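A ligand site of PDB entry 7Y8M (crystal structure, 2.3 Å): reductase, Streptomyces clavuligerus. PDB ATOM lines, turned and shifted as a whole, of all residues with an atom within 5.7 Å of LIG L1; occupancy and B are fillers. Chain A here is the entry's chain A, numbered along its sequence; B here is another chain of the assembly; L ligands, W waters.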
ATOM      1  N   GLY A  11      13.738  23.914 -19.766  1.00  0.00           N
ATOM      2  CA  GLY A  11      14.733  24.365 -18.786  1.00  0.00           C
ATOM      3  C   GLY A  11      15.879  25.054 -19.470  1.00  0.00           C
ATOM      4  O   GLY A  11      16.780  24.362 -19.919  1.00  0.00           O
ATOM      5  N   LEU A  12      15.840  26.373 -19.528  1.00  0.00           N
ATOM      6  CA  LEU A  12      16.844  27.124 -20.295  1.00  0.00           C
ATOM      7  C   LEU A  12      17.649  28.042 -19.376  1.00  0.00           C
ATOM      8  O   LEU A  12      17.770  29.235 -19.685  1.00  0.00           O
ATOM      9  CB  LEU A  12      16.113  27.885 -21.400  1.00  0.00           C
ATOM     10  CG  LEU A  12      15.417  27.014 -22.444  1.00  0.00           C
ATOM     11  CD1 LEU A  12      14.770  27.869 -23.510  1.00  0.00           C
ATOM     12  CD2 LEU A  12      16.408  26.053 -23.063  1.00  0.00           C
ATOM     13  N   GLY A  13      18.172  27.493 -18.298  1.00  0.00           N
ATOM     14  CA  GLY A  13      19.103  28.258 -17.454  1.00  0.00           C
ATOM     15  C   GLY A  13      20.498  28.124 -18.020  1.00  0.00           C
ATOM     16  O   GLY A  13      20.627  27.719 -19.171  1.00  0.00           O
ATOM     17  N   PRO A  14      21.597  28.420 -17.283  1.00  0.00           N
ATOM     18  CA  PRO A  14      22.928  28.338 -17.892  1.00  0.00           C
ATOM     19  C   PRO A  14      23.173  27.006 -18.635  1.00  0.00           C
ATOM     20  O   PRO A  14      23.714  27.055 -19.701  1.00  0.00           O
ATOM     21  CB  PRO A  14      23.852  28.493 -16.678  1.00  0.00           C
ATOM     22  CG  PRO A  14      23.107  29.376 -15.737  1.00  0.00           C
ATOM     23  CD  PRO A  14      21.697  28.877 -15.868  1.00  0.00           C
ATOM     24  N   MET A  15      22.738  25.886 -18.067  1.00  0.00           N
ATOM     25  CA  MET A  15      22.991  24.554 -18.670  1.00  0.00           C
ATOM     26  C   MET A  15      22.105  24.334 -19.898  1.00  0.00           C
ATOM     27  O   MET A  15      22.651  23.958 -20.930  1.00  0.00           O
ATOM     28  CB  MET A  15      22.732  23.446 -17.660  1.00  0.00           C
ATOM     29  CG  MET A  15      23.764  23.395 -16.569  1.00  0.00           C
ATOM     30  SD  MET A  15      25.435  23.140 -17.188  1.00  0.00           S
ATOM     31  CE  MET A  15      25.371  21.396 -17.557  1.00  0.00           C
ATOM     32  N   GLY A  16      20.817  24.589 -19.790  1.00  0.00           N
ATOM     33  CA  GLY A  16      19.879  24.400 -20.911  1.00  0.00           C
ATOM     34  C   GLY A  16      20.135  25.298 -22.110  1.00  0.00           C
ATOM     35  O   GLY A  16      19.984  24.821 -23.215  1.00  0.00           O
ATOM     36  N   ASN A  34      10.460  27.403 -21.718  1.00  0.00           N
ATOM     37  CA  ASN A  34      11.022  27.868 -20.432  1.00  0.00           C
ATOM     38  C   ASN A  34      10.027  28.766 -19.681  1.00  0.00           C
ATOM     39  O   ASN A  34       9.349  29.552 -20.340  1.00  0.00           O
ATOM     40  CB  ASN A  34      12.353  28.570 -20.605  1.00  0.00           C
ATOM     41  CG  ASN A  34      13.100  28.698 -19.298  1.00  0.00           C
ATOM     42  OD1 ASN A  34      13.457  27.704 -18.689  1.00  0.00           O
ATOM     43  ND2 ASN A  34      13.291  29.925 -18.850  1.00  0.00           N
ATOM     44  N   ARG A  35       9.941  28.611 -18.359  1.00  0.00           N
ATOM     45  CA  ARG A  35       9.047  29.453 -17.520  1.00  0.00           C
ATOM     46  C   ARG A  35       9.342  30.914 -17.832  1.00  0.00           C
ATOM     47  O   ARG A  35       8.379  31.634 -18.162  1.00  0.00           O
ATOM     48  CB  ARG A  35       9.239  29.063 -16.048  1.00  0.00           C
ATOM     49  CG  ARG A  35       8.816  30.114 -15.028  1.00  0.00           C
ATOM     50  CD  ARG A  35       9.116  29.630 -13.620  1.00  0.00           C
ATOM     51  NE  ARG A  35      10.543  29.624 -13.294  1.00  0.00           N
ATOM     52  CZ  ARG A  35      11.042  29.333 -12.104  1.00  0.00           C
ATOM     53  NH1 ARG A  35      10.247  29.015 -11.104  1.00  0.00           N
ATOM     54  NH2 ARG A  35      12.355  29.352 -11.925  1.00  0.00           N
ATOM     55  N   THR A  36      10.593  31.339 -17.750  1.00  0.00           N
ATOM     56  CA  THR A  36      10.937  32.707 -18.189  1.00  0.00           C
ATOM     57  C   THR A  36      11.025  32.663 -19.722  1.00  0.00           C
ATOM     58  O   THR A  36      12.074  32.296 -20.232  1.00  0.00           O
ATOM     59  CB  THR A  36      12.186  33.258 -17.494  1.00  0.00           C
ATOM     60  OG1 THR A  36      12.024  33.080 -16.081  1.00  0.00           O
ATOM     61  CG2 THR A  36      12.432  34.722 -17.780  1.00  0.00           C
ATOM     62  N   ARG A  39      14.240  33.669 -21.886  1.00  0.00           N
ATOM     63  CA  ARG A  39      15.476  32.860 -21.912  1.00  0.00           C
ATOM     64  C   ARG A  39      15.522  32.009 -23.189  1.00  0.00           C
ATOM     65  O   ARG A  39      16.564  31.427 -23.445  1.00  0.00           O
ATOM     66  CB  ARG A  39      15.590  31.997 -20.648  1.00  0.00           C
ATOM     67  CG  ARG A  39      15.578  32.782 -19.344  1.00  0.00           C
ATOM     68  CD  ARG A  39      16.958  33.315 -19.007  1.00  0.00           C
ATOM     69  NE  ARG A  39      17.955  32.257 -18.880  1.00  0.00           N
ATOM     70  CZ  ARG A  39      19.164  32.308 -19.414  1.00  0.00           C
ATOM     71  NH1 ARG A  39      19.530  33.348 -20.135  1.00  0.00           N
ATOM     72  NH2 ARG A  39      19.998  31.296 -19.237  1.00  0.00           N
ATOM     73  N   SER A  67      16.362  20.321 -17.954  1.00  0.00           N
ATOM     74  CA  SER A  67      17.495  20.885 -17.194  1.00  0.00           C
ATOM     75  C   SER A  67      16.925  21.843 -16.154  1.00  0.00           C
ATOM     76  O   SER A  67      16.792  23.029 -16.461  1.00  0.00           O
ATOM     77  CB  SER A  67      18.529  21.559 -18.065  1.00  0.00           C
ATOM     78  OG  SER A  67      19.559  22.138 -17.292  1.00  0.00           O
ATOM     79  N   LEU A  68      16.556  21.334 -14.994  1.00  0.00           N
ATOM     80  CA  LEU A  68      15.913  22.160 -13.955  1.00  0.00           C
ATOM     81  C   LEU A  68      16.690  22.100 -12.630  1.00  0.00           C
ATOM     82  O   LEU A  68      17.551  21.265 -12.518  1.00  0.00           O
ATOM     83  CB  LEU A  68      14.468  21.684 -13.770  1.00  0.00           C
ATOM     84  CG  LEU A  68      13.640  21.513 -15.045  1.00  0.00           C
ATOM     85  CD1 LEU A  68      12.424  20.645 -14.795  1.00  0.00           C
ATOM     86  CD2 LEU A  68      13.218  22.851 -15.610  1.00  0.00           C
ATOM     87  N   THR A  69      16.339  22.950 -11.667  1.00  0.00           N
ATOM     88  CA  THR A  69      17.042  23.031 -10.365  1.00  0.00           C
ATOM     89  C   THR A  69      16.956  21.708  -9.606  1.00  0.00           C
ATOM     90  O   THR A  69      17.963  21.295  -9.052  1.00  0.00           O
ATOM     91  CB  THR A  69      16.491  24.217  -9.551  1.00  0.00           C
ATOM     92  OG1 THR A  69      16.430  25.377 -10.371  1.00  0.00           O
ATOM     93  CG2 THR A  69      17.322  24.530  -8.328  1.00  0.00           C
ATOM     94  N   ASP A  70      15.782  21.071  -9.645  1.00  0.00           N
ATOM     95  CA  ASP A  70      15.543  19.817  -8.898  1.00  0.00           C
ATOM     96  C   ASP A  70      14.365  19.053  -9.519  1.00  0.00           C
ATOM     97  O   ASP A  70      13.791  19.544 -10.501  1.00  0.00           O
ATOM     98  CB  ASP A  70      15.300  20.101  -7.419  1.00  0.00           C
ATOM     99  CG  ASP A  70      14.212  21.111  -7.111  1.00  0.00           C
ATOM    100  OD1 ASP A  70      13.215  21.164  -7.844  1.00  0.00           O
ATOM    101  OD2 ASP A  70      14.347  21.810  -6.107  1.00  0.00           O
ATOM    102  N   ASP A  72      11.366  18.530  -8.062  1.00  0.00           N
ATOM    103  CA  ASP A  72      10.091  19.188  -7.707  1.00  0.00           C
ATOM    104  C   ASP A  72       9.670  20.097  -8.852  1.00  0.00           C
ATOM    105  O   ASP A  72       8.482  20.158  -9.148  1.00  0.00           O
ATOM    106  CB  ASP A  72      10.202  19.920  -6.377  1.00  0.00           C
ATOM    107  CG  ASP A  72       9.818  19.045  -5.193  1.00  0.00           C
ATOM    108  OD1 ASP A  72       8.879  18.242  -5.340  1.00  0.00           O
ATOM    109  OD2 ASP A  72      10.483  19.164  -4.148  1.00  0.00           O
ATOM    110  N   ALA A  73      10.645  20.741  -9.494  1.00  0.00           N
ATOM    111  CA  ALA A  73      10.371  21.591 -10.667  1.00  0.00           C
ATOM    112  C   ALA A  73       9.800  20.759 -11.808  1.00  0.00           C
ATOM    113  O   ALA A  73       9.012  21.307 -12.561  1.00  0.00           O
ATOM    114  CB  ALA A  73      11.658  22.258 -11.066  1.00  0.00           C
ATOM    115  N   ALA A  76       6.150  20.379 -11.066  1.00  0.00           N
ATOM    116  CA  ALA A  76       5.511  21.692 -11.281  1.00  0.00           C
ATOM    117  C   ALA A  76       5.262  21.972 -12.764  1.00  0.00           C
ATOM    118  O   ALA A  76       4.196  22.506 -13.080  1.00  0.00           O
ATOM    119  CB  ALA A  76       6.356  22.771 -10.671  1.00  0.00           C
ATOM    120  N   LEU A  77       6.188  21.580 -13.632  1.00  0.00           N
ATOM    121  CA  LEU A  77       6.059  21.907 -15.080  1.00  0.00           C
ATOM    122  C   LEU A  77       5.288  20.821 -15.841  1.00  0.00           C
ATOM    123  O   LEU A  77       4.457  21.191 -16.667  1.00  0.00           O
ATOM    124  CB  LEU A  77       7.461  22.067 -15.650  1.00  0.00           C
ATOM    125  CG  LEU A  77       8.127  23.406 -15.342  1.00  0.00           C
ATOM    126  CD1 LEU A  77       9.328  23.610 -16.240  1.00  0.00           C
ATOM    127  CD2 LEU A  77       7.125  24.534 -15.500  1.00  0.00           C
ATOM    128  N   LEU A  93      18.068  15.858 -16.523  1.00  0.00           N
ATOM    129  CA  LEU A  93      19.488  16.196 -16.260  1.00  0.00           C
ATOM    130  C   LEU A  93      19.544  17.123 -15.056  1.00  0.00           C
ATOM    131  O   LEU A  93      20.440  17.951 -14.974  1.00  0.00           O
ATOM    132  CB  LEU A  93      20.047  16.855 -17.515  1.00  0.00           C
ATOM    133  CG  LEU A  93      20.158  15.952 -18.740  1.00  0.00           C
ATOM    134  CD1 LEU A  93      20.832  16.688 -19.889  1.00  0.00           C
ATOM    135  CD2 LEU A  93      20.927  14.687 -18.411  1.00  0.00           C
ATOM    136  N   SER A  94      18.607  16.947 -14.131  1.00  0.00           N
ATOM    137  CA  SER A  94      18.506  17.821 -12.937  1.00  0.00           C
ATOM    138  C   SER A  94      19.052  17.102 -11.709  1.00  0.00           C
ATOM    139  O   SER A  94      18.852  15.899 -11.562  1.00  0.00           O
ATOM    140  CB  SER A  94      17.101  18.260 -12.736  1.00  0.00           C
ATOM    141  OG  SER A  94      16.515  18.711 -13.947  1.00  0.00           O
ATOM    142  N   SER A  95      19.741  17.852 -10.865  1.00  0.00           N
ATOM    143  CA  SER A  95      20.258  17.280  -9.614  1.00  0.00           C
ATOM    144  C   SER A  95      19.154  16.988  -8.616  1.00  0.00           C
ATOM    145  O   SER A  95      18.200  17.777  -8.555  1.00  0.00           O
ATOM    146  CB  SER A  95      21.288  18.173  -8.965  1.00  0.00           C
ATOM    147  OG  SER A  95      21.851  17.558  -7.810  1.00  0.00           O
ATOM    148  N   VAL A 120      25.118  15.768 -15.175  1.00  0.00           N
ATOM    149  CA  VAL A 120      26.127  16.379 -16.072  1.00  0.00           C
ATOM    150  C   VAL A 120      27.271  16.944 -15.223  1.00  0.00           C
ATOM    151  O   VAL A 120      27.025  17.831 -14.434  1.00  0.00           O
ATOM    152  CB  VAL A 120      25.487  17.426 -17.010  1.00  0.00           C
ATOM    153  CG1 VAL A 120      26.460  17.851 -18.083  1.00  0.00           C
ATOM    154  CG2 VAL A 120      24.201  16.909 -17.631  1.00  0.00           C
ATOM    155  N   THR A 121      28.476  16.415 -15.419  1.00  0.00           N
ATOM    156  CA  THR A 121      29.671  16.795 -14.624  1.00  0.00           C
ATOM    157  C   THR A 121      30.470  17.919 -15.289  1.00  0.00           C
ATOM    158  O   THR A 121      31.659  18.050 -14.995  1.00  0.00           O
ATOM    159  CB  THR A 121      30.528  15.534 -14.397  1.00  0.00           C
ATOM    160  OG1 THR A 121      31.071  15.079 -15.629  1.00  0.00           O
ATOM    161  CG2 THR A 121      29.745  14.423 -13.744  1.00  0.00           C
ATOM    162  N   CYS A 122      29.839  18.693 -16.154  1.00  0.00           N
ATOM    163  CA  CYS A 122      30.535  19.802 -16.846  1.00  0.00           C
ATOM    164  C   CYS A 122      29.801  21.117 -16.606  1.00  0.00           C
ATOM    165  O   CYS A 122      28.594  21.090 -16.354  1.00  0.00           O
ATOM    166  CB  CYS A 122      30.670  19.542 -18.342  1.00  0.00           C
ATOM    167  SG  CYS A 122      29.210  19.883 -19.342  1.00  0.00           S
ATOM    168  N   PRO A 123      30.480  22.299 -16.621  1.00  0.00           N
ATOM    169  CA  PRO A 123      29.781  23.570 -16.556  1.00  0.00           C
ATOM    170  C   PRO A 123      29.109  23.858 -17.906  1.00  0.00           C
ATOM    171  O   PRO A 123      29.316  23.118 -18.831  1.00  0.00           O
ATOM    172  CB  PRO A 123      30.904  24.571 -16.252  1.00  0.00           C
ATOM    173  CG  PRO A 123      32.079  24.012 -16.958  1.00  0.00           C
ATOM    174  CD  PRO A 123      31.960  22.556 -16.617  1.00  0.00           C
ATOM    175  N   PRO A 124      28.297  24.933 -18.076  1.00  0.00           N
ATOM    176  CA  PRO A 124      27.730  25.235 -19.389  1.00  0.00           C
ATOM    177  C   PRO A 124      28.777  25.328 -20.508  1.00  0.00           C
ATOM    178  O   PRO A 124      28.503  24.842 -21.558  1.00  0.00           O
ATOM    179  CB  PRO A 124      27.060  26.590 -19.157  1.00  0.00           C
ATOM    180  CG  PRO A 124      26.603  26.541 -17.749  1.00  0.00           C
ATOM    181  CD  PRO A 124      27.780  25.909 -17.074  1.00  0.00           C
ATOM    182  N   TYR A 170      26.802  11.726  -9.068  1.00  0.00           N
ATOM    183  CA  TYR A 170      26.869  13.202  -9.151  1.00  0.00           C
ATOM    184  C   TYR A 170      27.142  13.786  -7.759  1.00  0.00           C
ATOM    185  O   TYR A 170      28.007  14.639  -7.654  1.00  0.00           O
ATOM    186  CB  TYR A 170      25.603  13.790  -9.775  1.00  0.00           C
ATOM    187  CG  TYR A 170      25.688  15.260 -10.041  1.00  0.00           C
ATOM    188  CD1 TYR A 170      26.430  15.743 -11.105  1.00  0.00           C
ATOM    189  CD2 TYR A 170      25.067  16.173  -9.216  1.00  0.00           C
ATOM    190  CE1 TYR A 170      26.524  17.103 -11.352  1.00  0.00           C
ATOM    191  CE2 TYR A 170      25.142  17.530  -9.450  1.00  0.00           C
ATOM    192  CZ  TYR A 170      25.884  18.002 -10.524  1.00  0.00           C
ATOM    193  OH  TYR A 170      25.985  19.333 -10.751  1.00  0.00           O
ATOM    194  N   ALA B 232      26.733  31.734 -15.325  1.00  0.00           N
ATOM    195  CA  ALA B 232      27.194  30.336 -15.329  1.00  0.00           C
ATOM    196  C   ALA B 232      26.501  29.567 -14.207  1.00  0.00           C
ATOM    197  O   ALA B 232      26.389  28.339 -14.353  1.00  0.00           O
ATOM    198  CB  ALA B 232      28.689  30.301 -15.142  1.00  0.00           C
ATOM    199  N   ASP B 233      26.050  30.270 -13.170  1.00  0.00           N
ATOM    200  CA  ASP B 233      25.462  29.597 -11.992  1.00  0.00           C
ATOM    201  C   ASP B 233      24.666  30.564 -11.115  1.00  0.00           C
ATOM    202  O   ASP B 233      25.046  31.721 -11.032  1.00  0.00           O
ATOM    203  CB  ASP B 233      26.561  28.942 -11.155  1.00  0.00           C
ATOM    204  CG  ASP B 233      27.358  29.921 -10.316  1.00  0.00           C
ATOM    205  OD1 ASP B 233      28.189  30.634 -10.890  1.00  0.00           O
ATOM    206  OD2 ASP B 233      27.103  29.984  -9.116  1.00  0.00           O
ATOM    207  N   ARG B 234      23.644  30.055 -10.449  1.00  0.00           N
ATOM    208  CA  ARG B 234      22.871  30.873  -9.483  1.00  0.00           C
ATOM    209  C   ARG B 234      23.008  30.223  -8.103  1.00  0.00           C
ATOM    210  O   ARG B 234      23.074  28.999  -8.050  1.00  0.00           O
ATOM    211  CB  ARG B 234      21.398  30.933  -9.864  1.00  0.00           C
ATOM    212  CG  ARG B 234      21.067  31.785 -11.080  1.00  0.00           C
ATOM    213  CD  ARG B 234      19.685  31.424 -11.560  1.00  0.00           C
ATOM    214  NE  ARG B 234      18.619  31.725 -10.613  1.00  0.00           N
ATOM    215  CZ  ARG B 234      17.887  30.823  -9.959  1.00  0.00           C
ATOM    216  NH1 ARG B 234      18.108  29.523 -10.135  1.00  0.00           N
ATOM    217  NH2 ARG B 234      16.946  31.213  -9.130  1.00  0.00           N
ATOM    218  N   ALA B 236      20.830  29.894  -5.813  1.00  0.00           N
ATOM    219  CA  ALA B 236      19.637  29.060  -5.585  1.00  0.00           C
ATOM    220  C   ALA B 236      19.838  27.639  -6.141  1.00  0.00           C
ATOM    221  O   ALA B 236      19.451  26.707  -5.459  1.00  0.00           O
ATOM    222  CB  ALA B 236      18.435  29.718  -6.187  1.00  0.00           C
ATOM    223  N   MET B 237      20.397  27.519  -7.339  1.00  0.00           N
ATOM    224  CA  MET B 237      20.724  26.167  -7.871  1.00  0.00           C
ATOM    225  C   MET B 237      21.735  25.508  -6.922  1.00  0.00           C
ATOM    226  O   MET B 237      21.503  24.359  -6.560  1.00  0.00           O
ATOM    227  CB  MET B 237      21.292  26.273  -9.293  1.00  0.00           C
ATOM    228  CG  MET B 237      21.722  24.977  -9.909  1.00  0.00           C
ATOM    229  SD  MET B 237      23.458  24.572  -9.628  1.00  0.00           S
ATOM    230  CE  MET B 237      24.256  26.069 -10.185  1.00  0.00           C
ATOM    231  N   SER B 241      21.642  22.049  -4.772  1.00  0.00           N
ATOM    232  CA  SER B 241      22.734  21.058  -4.949  1.00  0.00           C
ATOM    233  C   SER B 241      23.299  20.594  -3.595  1.00  0.00           C
ATOM    234  O   SER B 241      23.428  19.398  -3.408  1.00  0.00           O
ATOM    235  CB  SER B 241      23.809  21.618  -5.865  1.00  0.00           C
ATOM    236  OG  SER B 241      24.943  20.785  -5.928  1.00  0.00           O
ATOM    237  N   HIS B 244      20.901  18.518  -1.784  1.00  0.00           N
ATOM    238  CA  HIS B 244      20.880  17.145  -2.343  1.00  0.00           C
ATOM    239  C   HIS B 244      22.004  16.344  -1.720  1.00  0.00           C
ATOM    240  O   HIS B 244      21.764  15.204  -1.407  1.00  0.00           O
ATOM    241  CB  HIS B 244      20.926  17.185  -3.871  1.00  0.00           C
ATOM    242  CG  HIS B 244      19.859  18.005  -4.501  1.00  0.00           C
ATOM    243  ND1 HIS B 244      20.058  18.711  -5.652  1.00  0.00           N
ATOM    244  CD2 HIS B 244      18.588  18.240  -4.133  1.00  0.00           C
ATOM    245  CE1 HIS B 244      18.966  19.343  -5.975  1.00  0.00           C
ATOM    246  NE2 HIS B 244      18.041  19.067  -5.071  1.00  0.00           N
HETATM  247  P1  LIG L   1      19.066  26.755 -12.648  1.00  0.00           P
HETATM  248  O1  LIG L   1      18.725  26.198 -11.320  1.00  0.00           O
HETATM  249  O2  LIG L   1      19.707  28.092 -12.700  1.00  0.00           O
HETATM  250  O3  LIG L   1      17.765  26.794 -13.544  1.00  0.00           O
HETATM  251  C1  LIG L   1      17.477  25.709 -14.435  1.00  0.00           C
HETATM  252  C2  LIG L   1      16.059  25.849 -14.935  1.00  0.00           C
HETATM  253  O4  LIG L   1      15.143  25.402 -13.919  1.00  0.00           O
HETATM  254  C3  LIG L   1      15.607  27.262 -15.325  1.00  0.00           C
HETATM  255  O5  LIG L   1      15.212  27.256 -16.686  1.00  0.00           O
HETATM  256  C4  LIG L   1      14.461  27.570 -14.358  1.00  0.00           C
HETATM  257  O6  LIG L   1      13.400  28.319 -14.948  1.00  0.00           O
HETATM  258  C5  LIG L   1      13.976  26.162 -14.043  1.00  0.00           C
HETATM  259  N1  LIG L   1      13.193  26.016 -12.825  1.00  0.00           N
HETATM  260  C6  LIG L   1      13.656  25.911 -11.541  1.00  0.00           C
HETATM  261  N2  LIG L   1      12.707  25.784 -10.656  1.00  0.00           N
HETATM  262  C7  LIG L   1      11.541  25.802 -11.397  1.00  0.00           C
HETATM  263  C8  LIG L   1      10.184  25.711 -11.035  1.00  0.00           C
HETATM  264  N3  LIG L   1       9.752  25.565  -9.791  1.00  0.00           N
HETATM  265  N4  LIG L   1       9.267  25.757 -12.030  1.00  0.00           N
HETATM  266  C9  LIG L   1       9.709  25.903 -13.286  1.00  0.00           C
HETATM  267  N5  LIG L   1      10.941  25.997 -13.743  1.00  0.00           N
HETATM  268  C10 LIG L   1      11.830  25.937 -12.745  1.00  0.00           C
HETATM  269  O7  LIG L   1      19.946  25.637 -13.362  1.00  0.00           O
HETATM  270  P2  LIG L   1      21.275  25.425 -14.221  1.00  0.00           P
HETATM  271  O8  LIG L   1      20.965  25.685 -15.646  1.00  0.00           O
HETATM  272  O9  LIG L   1      22.409  26.142 -13.594  1.00  0.00           O
HETATM  273  O10 LIG L   1      21.469  23.865 -14.019  1.00  0.00           O
HETATM  274  C11 LIG L   1      20.325  22.990 -14.100  1.00  0.00           C
HETATM  275  C12 LIG L   1      20.627  21.704 -13.380  1.00  0.00           C
HETATM  276  O11 LIG L   1      21.889  21.176 -13.845  1.00  0.00           O
HETATM  277  C13 LIG L   1      20.713  21.804 -11.850  1.00  0.00           C
HETATM  278  O12 LIG L   1      19.966  20.769 -11.233  1.00  0.00           O
HETATM  279  C14 LIG L   1      22.215  21.729 -11.583  1.00  0.00           C
HETATM  280  O13 LIG L   1      22.513  21.095 -10.364  1.00  0.00           O
HETATM  281  C15 LIG L   1      22.770  20.952 -12.774  1.00  0.00           C
HETATM  282  N6  LIG L   1      24.116  21.416 -13.188  1.00  0.00           N
HETATM  283  C16 LIG L   1      24.521  22.717 -13.059  1.00  0.00           C
HETATM  284  C17 LIG L   1      25.745  23.133 -13.528  1.00  0.00           C
HETATM  285  C18 LIG L   1      26.063  24.566 -13.692  1.00  0.00           C
HETATM  286  O14 LIG L   1      27.236  24.891 -13.862  1.00  0.00           O
HETATM  287  N7  LIG L   1      25.097  25.465 -13.671  1.00  0.00           N
HETATM  288  C19 LIG L   1      26.750  22.111 -13.866  1.00  0.00           C
HETATM  289  C20 LIG L   1      26.257  20.744 -13.802  1.00  0.00           C
HETATM  290  C21 LIG L   1      24.975  20.505 -13.750  1.00  0.00           C
HETATM  291  P3  LIG L   1      13.690  29.890 -15.171  1.00  0.00           P
HETATM  292  O15 LIG L   1      12.314  30.478 -15.297  1.00  0.00           O
HETATM  293  O16 LIG L   1      14.470  30.086 -16.429  1.00  0.00           O
HETATM  294  O17 LIG L   1      14.422  30.442 -13.967  1.00  0.00           O
HETATM  295  C1  LG2 L   2      29.598  24.570 -11.503  1.00  0.00           C
HETATM  296  C2  LG2 L   2      28.786  25.535 -10.675  1.00  0.00           C
HETATM  297  C3  LG2 L   2      29.165  23.300 -11.175  1.00  0.00           C
HETATM  298  C4  LG2 L   2      27.687  24.691 -10.117  1.00  0.00           C
HETATM  299  C5  LG2 L   2      29.792  22.183 -11.555  1.00  0.00           C
HETATM  300  C6  LG2 L   2      31.125  22.230 -11.914  1.00  0.00           C
HETATM  301  C7  LG2 L   2      29.147  20.946 -11.574  1.00  0.00           C
HETATM  302  C8  LG2 L   2      29.828  19.806 -11.951  1.00  0.00           C
HETATM  303  C9  LG2 L   2      31.809  21.080 -12.281  1.00  0.00           C
HETATM  304  C10 LG2 L   2      31.160  19.873 -12.299  1.00  0.00           C
HETATM  305  F1  LG2 L   2      29.255  18.712 -11.960  1.00  0.00           F
HETATM  306  N1  LG2 L   2      28.092  23.308 -10.386  1.00  0.00           N
HETATM  307  O   HOH W   1      21.566  20.139 -16.244  1.00  0.00           O
HETATM  308  O   HOH W   2      19.066  25.068 -17.369  1.00  0.00           O
HETATM  309  O   HOH W   3      20.668  22.272  -8.432  1.00  0.00           O
HETATM  310  O   HOH W   4      16.865  31.016 -16.626  1.00  0.00           O
HETATM  311  O   HOH W   5       6.440  26.266 -12.448  1.00  0.00           O
HETATM  312  O   HOH W   6      24.958  21.249  -9.059  1.00  0.00           O
HETATM  313  O   HOH W   7      11.400  26.377 -17.008  1.00  0.00           O
HETATM  314  O   HOH W   8      22.145  28.181 -12.008  1.00  0.00           O
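Water W8 lies within hydrogen-bond range of an oxygen (O2) of LIG L1 (2.5 Å) and the backbone NH (N) of Arg 234 of chain B (2.9 Å).
Water W4 lies within hydrogen-bond range of O16 of LIG L1 and NE of Arg 39.
Water W1 lies within hydrogen-bond range of an oxygen (O11) of LIG L1, the backbone carbonyl oxygen of Leu 93 and the side-chain hydroxyl of Ser 67.
Water W2 lies within hydrogen-bond range of an oxygen (O8) of LIG L1, the backbone NH (N) of Gly 13, the side-chain hydroxyl (OG) of Ser 67, the backbone NH (N) of Gly 16 and the backbone carbonyl oxygen (O) of Gly 11.
Water W6 lies within hydrogen-bond range of OH of Tyr 170 (2.8 Å), O13 of LIG L1 (2.8 Å), OG of Ser 241 of chain B (3.2 Å) and SD of Met 237 of chain B (3.7 Å).
Water W3 lies within hydrogen-bond range of an oxygen (O13) of LIG L1, the backbone carbonyl oxygen (O) of Met 237 of chain B and the backbone carbonyl oxygen (O) of Thr 69.
O12 of LIG L1 sits at hydrogen-bond distance from O of Thr 69, at 3.0 Å.
OG1 of Thr 69 lies within hydrogen-bond range of O1 of LIG L1, at 2.6 Å.
O16 of LIG L1 lies within hydrogen-bond range of ND2 of Asn 34.
N of Thr 36 is in hydrogen-bond range of O15 of LIG L1 (3.1 Å).
OG1 of Thr 36 is in hydrogen-bond range of O15 of LIG L1 (2.7 Å).
The backbone carbonyl oxygen (O) of Leu 68 is in hydrogen-bond range of an oxygen (O12) of LIG L1 (2.8 Å).
NE of Arg 35 lies within salt-bridge range of O15 of LIG L1 (2.8 Å).
O12 of LIG L1 lies within hydrogen-bond range of N of Ser 95.
N of Met 15 is in hydrogen-bond range of O8 of LIG L1 (3.0 Å).
N of Leu 12 sits at hydrogen-bond distance from O5 of LIG L1, at 3.0 Å.
A nitrogen (N7) of LIG L1 lies within hydrogen-bond range of the backbone carbonyl oxygen (O) of Ala 232 of chain B (3.2 Å).
The side-chain sulfur of Met 237 of chain B sits close to an oxygen (O13) of LIG L1 (3.7 Å).
O2 of LIG L1 lies within salt-bridge range of NH1 of Arg 234 of chain B.
The backbone NH (N) of Gly 13 sits at hydrogen-bond distance from an oxygen (O5) of LIG L1 (3.4 Å).
An oxygen (O8) of LIG L1 lies close to the backbone nitrogen (N) of Pro 14 (3.2 Å).
Gly 11 touches LIG L1.
Ser 67 touches LIG L1.
Ala 73 touches LIG L1 (CB to C7, 3.6 Å).
Leu 77 touches LIG L1 (CG to C9, 3.6 Å).
Leu 93 touches LIG L1 (O to O11, 3.7 Å).
CA of Ser 94 touches O12 of LIG L1, 3.7 Å away.
O of Val 120 touches C20 of LIG L1, 3.1 Å away.
O of Cys 122 touches C19 of LIG L1, at 3.3 Å.
Pro 123 touches LIG L1 (CA to O14, 3.9 Å).
Pro 124 touches LIG L1 (CD to O14, 3.4 Å).
OH of Tyr 170 touches C20 of LIG L1, 3.4 Å away.
Hydrophobic or aromatic side chains within 4 Å of LIG L1: Pro 14, Met 15, Leu 68, Ala 73, Leu 77, Pro 124 and Met 237 of chain B.
Of the 34 residues printed, 24 come within 4 Å of LIG L1.
The backbone carbonyl oxygen (O) of Thr 36 lies within hydrogen-bond range of the side-chain amide nitrogen (ND2) of Asn 34, 3.0 Å away.
The side-chain amide oxygen (OD1) of Asn 34 sits at hydrogen-bond distance from the backbone NH (N) of Leu 12 (2.9 Å).
The backbone NH (N) of Leu 68 sits at hydrogen-bond distance from the side-chain hydroxyl (OG) of Ser 94.
ND1 of His 244 of chain B sits at hydrogen-bond distance from OG of Ser 95 (3.0 Å).
The backbone carbonyl oxygen (O) of Leu 12 lies within hydrogen-bond range of the guanidinium group (NH2) of Arg 39 (3.1 Å).
The backbone NH (N) of Ala 73 lies within hydrogen-bond range of the side-chain carboxylate (OD1) of Asp 70 (3.1 Å).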
